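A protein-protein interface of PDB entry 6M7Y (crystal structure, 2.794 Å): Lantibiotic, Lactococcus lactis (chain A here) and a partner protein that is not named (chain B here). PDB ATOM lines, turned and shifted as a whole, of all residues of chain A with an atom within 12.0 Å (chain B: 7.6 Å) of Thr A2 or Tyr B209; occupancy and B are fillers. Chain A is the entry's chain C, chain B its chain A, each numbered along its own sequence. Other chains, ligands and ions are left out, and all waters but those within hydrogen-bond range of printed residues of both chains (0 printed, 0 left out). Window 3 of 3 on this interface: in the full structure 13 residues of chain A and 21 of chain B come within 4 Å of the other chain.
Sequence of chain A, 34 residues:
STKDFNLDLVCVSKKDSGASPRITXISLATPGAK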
ATOM      1  N   THR A   2      11.626  20.925  22.891  1.00  0.00           N
ATOM      2  CA  THR A   2      12.445  20.050  22.062  1.00  0.00           C
ATOM      3  C   THR A   2      12.356  18.629  22.594  1.00  0.00           C
ATOM      4  O   THR A   2      11.401  18.277  23.278  1.00  0.00           O
ATOM      5  CB  THR A   2      13.920  20.507  22.029  1.00  0.00           C
ATOM      6  N   LYS A   3      13.343  17.804  22.265  1.00  0.00           N
ATOM      7  CA  LYS A   3      13.458  16.461  22.841  1.00  0.00           C
ATOM      8  C   LYS A   3      14.393  16.460  24.043  1.00  0.00           C
ATOM      9  O   LYS A   3      15.330  15.667  24.111  1.00  0.00           O
ATOM     10  CB  LYS A   3      13.936  15.460  21.794  1.00  0.00           C
ATOM     11  CG  LYS A   3      13.074  15.299  20.537  1.00  0.00           C
ATOM     12  CD  LYS A   3      11.609  15.553  20.805  1.00  0.00           C
ATOM     13  CE  LYS A   3      11.157  16.856  20.187  1.00  0.00           C
ATOM     14  NZ  LYS A   3       9.773  17.161  20.632  1.00  0.00           N
ATOM     15  N   ASP A   4      14.194  17.374  24.997  1.00  0.00           N
ATOM     16  CA  ASP A   4      14.709  17.160  26.341  1.00  0.00           C
ATOM     17  C   ASP A   4      13.632  16.573  27.240  1.00  0.00           C
ATOM     18  O   ASP A   4      13.578  16.838  28.449  1.00  0.00           O
ATOM     19  CB  ASP A   4      15.349  18.423  26.940  1.00  0.00           C
ATOM     20  CG  ASP A   4      14.581  19.687  26.666  1.00  0.00           C
ATOM     21  OD1 ASP A   4      13.345  19.663  26.788  1.00  0.00           O
ATOM     22  OD2 ASP A   4      15.225  20.720  26.356  1.00  0.00           O
ATOM     23  N   PHE A   5      12.768  15.760  26.640  1.00  0.00           N
ATOM     24  CA  PHE A   5      11.952  14.794  27.351  1.00  0.00           C
ATOM     25  C   PHE A   5      12.542  13.382  27.289  1.00  0.00           C
ATOM     26  O   PHE A   5      11.823  12.413  27.590  1.00  0.00           O
ATOM     27  CB  PHE A   5      10.530  14.785  26.784  1.00  0.00           C
ATOM     28  CG  PHE A   5       9.747  16.027  27.067  1.00  0.00           C
ATOM     29  CD1 PHE A   5       9.964  17.182  26.335  1.00  0.00           C
ATOM     30  CD2 PHE A   5       8.767  16.033  28.054  1.00  0.00           C
ATOM     31  CE1 PHE A   5       9.243  18.331  26.599  1.00  0.00           C
ATOM     32  CE2 PHE A   5       8.028  17.175  28.327  1.00  0.00           C
ATOM     33  CZ  PHE A   5       8.262  18.329  27.597  1.00  0.00           C
ATOM     34  N   ASN A   6      13.831  13.244  26.905  1.00  0.00           N
ATOM     35  CA  ASN A   6      14.423  11.926  26.632  1.00  0.00           C
ATOM     36  C   ASN A   6      14.382  11.011  27.851  1.00  0.00           C
ATOM     37  O   ASN A   6      13.485  10.171  27.952  1.00  0.00           O
ATOM     38  CB  ASN A   6      15.881  12.017  26.152  1.00  0.00           C
ATOM     39  CG  ASN A   6      16.437  10.661  25.618  1.00  0.00           C
ATOM     40  OD1 ASN A   6      15.890   9.590  25.869  1.00  0.00           O
ATOM     41  ND2 ASN A   6      17.519  10.740  24.833  1.00  0.00           N
ATOM     42  N   LEU A   7      15.359  11.164  28.746  1.00  0.00           N
ATOM     43  CA  LEU A   7      15.601  10.369  29.958  1.00  0.00           C
ATOM     44  C   LEU A   7      16.888   9.591  29.797  1.00  0.00           C
ATOM     45  O   LEU A   7      17.700   9.540  30.725  1.00  0.00           O
ATOM     46  CB  LEU A   7      14.492   9.375  30.305  1.00  0.00           C
ATOM     47  CG  LEU A   7      14.673   8.583  31.591  1.00  0.00           C
ATOM     48  CD1 LEU A   7      14.146   9.381  32.772  1.00  0.00           C
ATOM     49  CD2 LEU A   7      14.003   7.198  31.542  1.00  0.00           C
ATOM     50  N   ASN B 178      16.160  19.620  30.691  1.00  0.00           N
ATOM     51  CA  ASN B 178      15.329  20.726  31.136  1.00  0.00           C
ATOM     52  C   ASN B 178      14.064  20.226  31.829  1.00  0.00           C
ATOM     53  O   ASN B 178      13.616  20.824  32.814  1.00  0.00           O
ATOM     54  CB  ASN B 178      14.995  21.632  29.961  1.00  0.00           C
ATOM     55  CG  ASN B 178      16.142  22.552  29.608  1.00  0.00           C
ATOM     56  OD1 ASN B 178      17.001  22.828  30.441  1.00  0.00           O
ATOM     57  ND2 ASN B 178      16.165  23.033  28.375  1.00  0.00           N
ATOM     58  N   VAL B 179      13.515  19.100  31.390  1.00  0.00           N
ATOM     59  CA  VAL B 179      12.276  18.646  31.998  1.00  0.00           C
ATOM     60  C   VAL B 179      12.519  17.990  33.352  1.00  0.00           C
ATOM     61  O   VAL B 179      11.675  18.090  34.253  1.00  0.00           O
ATOM     62  CB  VAL B 179      11.536  17.713  31.037  1.00  0.00           C
ATOM     63  CG1 VAL B 179      10.216  17.272  31.683  1.00  0.00           C
ATOM     64  CG2 VAL B 179      11.296  18.445  29.738  1.00  0.00           C
ATOM     65  N   CYS B 198       2.410  17.951  35.869  1.00  0.00           N
ATOM     66  CA  CYS B 198       2.152  18.001  34.427  1.00  0.00           C
ATOM     67  C   CYS B 198       1.944  19.423  33.923  1.00  0.00           C
ATOM     68  O   CYS B 198       2.461  19.795  32.861  1.00  0.00           O
ATOM     69  CB  CYS B 198       0.927  17.167  34.089  1.00  0.00           C
ATOM     70  SG  CYS B 198       1.259  15.442  33.966  1.00  0.00           S
ATOM     71  N   VAL B 201       5.028  21.661  33.548  1.00  0.00           N
ATOM     72  CA  VAL B 201       5.846  21.310  32.386  1.00  0.00           C
ATOM     73  C   VAL B 201       5.293  21.955  31.119  1.00  0.00           C
ATOM     74  O   VAL B 201       6.028  22.616  30.370  1.00  0.00           O
ATOM     75  CB  VAL B 201       5.950  19.776  32.234  1.00  0.00           C
ATOM     76  CG1 VAL B 201       6.788  19.386  31.014  1.00  0.00           C
ATOM     77  CG2 VAL B 201       6.535  19.153  33.474  1.00  0.00           C
ATOM     78  N   THR B 202       3.996  21.758  30.846  1.00  0.00           N
ATOM     79  CA  THR B 202       3.419  22.285  29.611  1.00  0.00           C
ATOM     80  C   THR B 202       3.410  23.804  29.609  1.00  0.00           C
ATOM     81  O   THR B 202       3.590  24.424  28.555  1.00  0.00           O
ATOM     82  CB  THR B 202       1.997  21.754  29.414  1.00  0.00           C
ATOM     83  OG1 THR B 202       1.259  21.900  30.633  1.00  0.00           O
ATOM     84  CG2 THR B 202       2.023  20.290  29.036  1.00  0.00           C
ATOM     85  N   CYS B 204       5.544  25.881  30.270  1.00  0.00           N
ATOM     86  CA  CYS B 204       6.688  26.472  29.585  1.00  0.00           C
ATOM     87  C   CYS B 204       7.227  25.535  28.518  1.00  0.00           C
ATOM     88  O   CYS B 204       8.437  25.442  28.301  1.00  0.00           O
ATOM     89  CB  CYS B 204       7.795  26.887  30.560  1.00  0.00           C
ATOM     90  SG  CYS B 204       8.481  25.612  31.618  1.00  0.00           S
ATOM     91  N   TYR B 205       6.320  24.828  27.846  1.00  0.00           N
ATOM     92  CA  TYR B 205       6.635  24.089  26.627  1.00  0.00           C
ATOM     93  C   TYR B 205       5.506  24.243  25.616  1.00  0.00           C
ATOM     94  O   TYR B 205       5.752  24.415  24.419  1.00  0.00           O
ATOM     95  CB  TYR B 205       6.892  22.604  26.923  1.00  0.00           C
ATOM     96  CG  TYR B 205       8.335  22.300  27.279  1.00  0.00           C
ATOM     97  CD1 TYR B 205       9.295  22.169  26.288  1.00  0.00           C
ATOM     98  CD2 TYR B 205       8.741  22.165  28.605  1.00  0.00           C
ATOM     99  CE1 TYR B 205      10.626  21.919  26.601  1.00  0.00           C
ATOM    100  CE2 TYR B 205      10.077  21.906  28.928  1.00  0.00           C
ATOM    101  CZ  TYR B 205      11.012  21.784  27.920  1.00  0.00           C
ATOM    102  OH  TYR B 205      12.337  21.527  28.214  1.00  0.00           O
ATOM    103  N   GLY B 206       4.268  24.214  26.105  1.00  0.00           N
ATOM    104  CA  GLY B 206       3.072  24.212  25.276  1.00  0.00           C
ATOM    105  C   GLY B 206       2.152  23.073  25.675  1.00  0.00           C
ATOM    106  O   GLY B 206       2.619  22.086  26.249  1.00  0.00           O
ATOM    107  N   ASP B 207       0.850  23.180  25.401  1.00  0.00           N
ATOM    108  CA  ASP B 207      -0.028  22.045  25.680  1.00  0.00           C
ATOM    109  C   ASP B 207       0.163  20.923  24.672  1.00  0.00           C
ATOM    110  O   ASP B 207      -0.284  19.798  24.925  1.00  0.00           O
ATOM    111  CB  ASP B 207      -1.481  22.498  25.725  1.00  0.00           C
ATOM    112  CG  ASP B 207      -1.754  23.434  26.896  1.00  0.00           C
ATOM    113  OD1 ASP B 207      -1.413  23.077  28.054  1.00  0.00           O
ATOM    114  OD2 ASP B 207      -2.279  24.545  26.652  1.00  0.00           O
ATOM    115  N   GLU B 208       0.848  21.217  23.555  1.00  0.00           N
ATOM    116  CA  GLU B 208       1.286  20.205  22.589  1.00  0.00           C
ATOM    117  C   GLU B 208       2.031  19.052  23.258  1.00  0.00           C
ATOM    118  O   GLU B 208       1.965  17.905  22.791  1.00  0.00           O
ATOM    119  CB  GLU B 208       2.207  20.863  21.554  1.00  0.00           C
ATOM    120  CG  GLU B 208       2.222  22.395  21.665  1.00  0.00           C
ATOM    121  CD  GLU B 208       3.338  23.049  20.851  1.00  0.00           C
ATOM    122  OE1 GLU B 208       3.678  24.218  21.158  1.00  0.00           O
ATOM    123  OE2 GLU B 208       3.879  22.397  19.919  1.00  0.00           O
ATOM    124  N   TYR B 209       2.748  19.344  24.346  1.00  0.00           N
ATOM    125  CA  TYR B 209       3.694  18.431  24.969  1.00  0.00           C
ATOM    126  C   TYR B 209       3.098  17.635  26.122  1.00  0.00           C
ATOM    127  O   TYR B 209       3.843  16.960  26.839  1.00  0.00           O
ATOM    128  CB  TYR B 209       4.910  19.214  25.470  1.00  0.00           C
ATOM    129  CG  TYR B 209       5.828  19.711  24.385  1.00  0.00           C
ATOM    130  CD1 TYR B 209       6.875  18.923  23.925  1.00  0.00           C
ATOM    131  CD2 TYR B 209       5.651  20.962  23.817  1.00  0.00           C
ATOM    132  CE1 TYR B 209       7.734  19.366  22.933  1.00  0.00           C
ATOM    133  CE2 TYR B 209       6.506  21.417  22.822  1.00  0.00           C
ATOM    134  CZ  TYR B 209       7.545  20.609  22.387  1.00  0.00           C
ATOM    135  OH  TYR B 209       8.398  21.042  21.404  1.00  0.00           O
ATOM    136  N   ARG B 210       1.785  17.704  26.325  1.00  0.00           N
ATOM    137  CA  ARG B 210       1.188  17.069  27.492  1.00  0.00           C
ATOM    138  C   ARG B 210       1.348  15.544  27.447  1.00  0.00           C
ATOM    139  O   ARG B 210       1.503  14.906  28.496  1.00  0.00           O
ATOM    140  CB  ARG B 210      -0.278  17.500  27.591  1.00  0.00           C
ATOM    141  CG  ARG B 210      -1.137  16.649  28.482  1.00  0.00           C
ATOM    142  CD  ARG B 210      -0.942  17.062  29.911  1.00  0.00           C
ATOM    143  NE  ARG B 210      -1.674  16.173  30.793  1.00  0.00           N
ATOM    144  CZ  ARG B 210      -2.269  16.561  31.912  1.00  0.00           C
ATOM    145  NH1 ARG B 210      -2.199  17.832  32.292  1.00  0.00           N
ATOM    146  NH2 ARG B 210      -2.911  15.665  32.666  1.00  0.00           N
ATOM    147  N   GLU B 211       1.331  14.953  26.246  1.00  0.00           N
ATOM    148  CA  GLU B 211       1.670  13.541  26.079  1.00  0.00           C
ATOM    149  C   GLU B 211       2.994  13.218  26.763  1.00  0.00           C
ATOM    150  O   GLU B 211       3.039  12.483  27.761  1.00  0.00           O
ATOM    151  CB  GLU B 211       1.739  13.206  24.582  1.00  0.00           C
ATOM    152  CG  GLU B 211       2.615  14.212  23.795  1.00  0.00           C
ATOM    153  CD  GLU B 211       3.356  13.621  22.588  1.00  0.00           C
ATOM    154  OE1 GLU B 211       3.350  12.387  22.399  1.00  0.00           O
ATOM    155  OE2 GLU B 211       3.996  14.404  21.848  1.00  0.00           O
ATOM    156  N   LEU B 212       4.074  13.821  26.248  1.00  0.00           N
ATOM    157  CA  LEU B 212       5.439  13.555  26.691  1.00  0.00           C
ATOM    158  C   LEU B 212       5.616  13.810  28.184  1.00  0.00           C
ATOM    159  O   LEU B 212       6.267  13.021  28.885  1.00  0.00           O
ATOM    160  CB  LEU B 212       6.395  14.439  25.894  1.00  0.00           C
ATOM    161  CG  LEU B 212       6.264  14.268  24.386  1.00  0.00           C
ATOM    162  CD1 LEU B 212       6.977  15.399  23.663  1.00  0.00           C
ATOM    163  CD2 LEU B 212       6.789  12.895  23.953  1.00  0.00           C
ATOM    164  N   SER B 213       5.080  14.929  28.674  1.00  0.00           N
ATOM    165  CA  SER B 213       5.165  15.246  30.091  1.00  0.00           C
ATOM    166  C   SER B 213       4.708  14.071  30.923  1.00  0.00           C
ATOM    167  O   SER B 213       5.406  13.630  31.842  1.00  0.00           O
ATOM    168  CB  SER B 213       4.308  16.469  30.394  1.00  0.00           C
ATOM    169  OG  SER B 213       4.370  17.358  29.305  1.00  0.00           O
ATOM    170  N   GLU B 214       3.545  13.528  30.591  1.00  0.00           N
ATOM    171  CA  GLU B 214       3.009  12.438  31.388  1.00  0.00           C
ATOM    172  C   GLU B 214       3.916  11.221  31.314  1.00  0.00           C
ATOM    173  O   GLU B 214       4.231  10.607  32.343  1.00  0.00           O
ATOM    174  CB  GLU B 214       1.592  12.111  30.918  1.00  0.00           C
ATOM    175  CG  GLU B 214       0.586  13.221  31.237  1.00  0.00           C
ATOM    176  CD  GLU B 214      -0.832  12.920  30.763  1.00  0.00           C
ATOM    177  OE1 GLU B 214      -1.009  11.976  29.956  1.00  0.00           O
ATOM    178  OE2 GLU B 214      -1.773  13.614  31.229  1.00  0.00           O
ATOM    179  N   GLN B 215       4.367  10.876  30.109  1.00  0.00           N
ATOM    180  CA  GLN B 215       5.298   9.771  29.954  1.00  0.00           C
ATOM    181  C   GLN B 215       6.576  10.016  30.749  1.00  0.00           C
ATOM    182  O   GLN B 215       6.971   9.194  31.590  1.00  0.00           O
ATOM    183  CB  GLN B 215       5.616   9.564  28.479  1.00  0.00           C
ATOM    184  CG  GLN B 215       4.475   9.063  27.655  1.00  0.00           C
ATOM    185  CD  GLN B 215       4.943   8.616  26.292  1.00  0.00           C
ATOM    186  OE1 GLN B 215       4.151   8.485  25.361  1.00  0.00           O
ATOM    187  NE2 GLN B 215       6.253   8.375  26.169  1.00  0.00           N
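Printed residues of chain B within 4 Å of Lys A3: Tyr B209 (3.8 Å). Printed residues of chain A within 4 Å of Asn B178: Asp A4 (3.2 Å). Printed residues of chain A within 4 Å of Val B201: Phe A5 (3.7 Å). No residue of chain A comes within 4 Å of Thr B202. Of chain A, only Thr A2 (3.97 Å), Asp A4 (2.6 Å) and Phe A5 (3.8 Å) come within 4 Å of Tyr B205. Gly B206 touches none of the printed residues of chain A. No residue of chain A comes within 4 Å of Asp B207. Tyr B209 touches three residues of chain A. No residue of chain A comes within 4 Å of Glu B211. The nearest residue of chain B that does not touch Thr A2 is Leu B212 (5.3 Å).
The side-chain hydroxyl of Ser B213 lies within hydrogen-bond range of the backbone carbonyl oxygen of Tyr B209 (2.6 Å).
Hydrophobic or aromatic side chains of chain A that line the printed part of chain B: Phe A5. Of the 17 printed residues of chain B, 7 touch a printed residue of chain A. Printed residues of chain B that touch a printed residue of chain A: Asn B178, Val B179, Val B201, Tyr B205, Tyr B209, Leu B212 and Ser B213. Hydrophobic or aromatic side chains of chain B within 4 Å of the printed part of chain A: Val B179, Val B201, Tyr B205, Tyr B209 and Leu B212. Among the printed residues, 12 pairs touch across the chains.
Among the printed residues, pairs that only touch across the chains: Asp A4 with Val B179, Thr A2 with Tyr B209, Phe A5 with Leu B212, Phe A5 with Tyr B209, Phe A5 with Val B201, Phe A5 with Val B179, Phe A5 with Ser B213, Lys A3 with Tyr B209, Phe A5 with Tyr B205 and Thr A2 with Tyr B205.
The side-chain hydroxyl (OH) of Tyr B205 lies within hydrogen-bond range of the side-chain carboxylate (OD1) of Asp A4 (2.6 Å). The side-chain amide nitrogen (ND2) of Asn B178 lies within hydrogen-bond range of the side-chain carboxylate (OD2) of Asp A4, 3.2 Å away.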
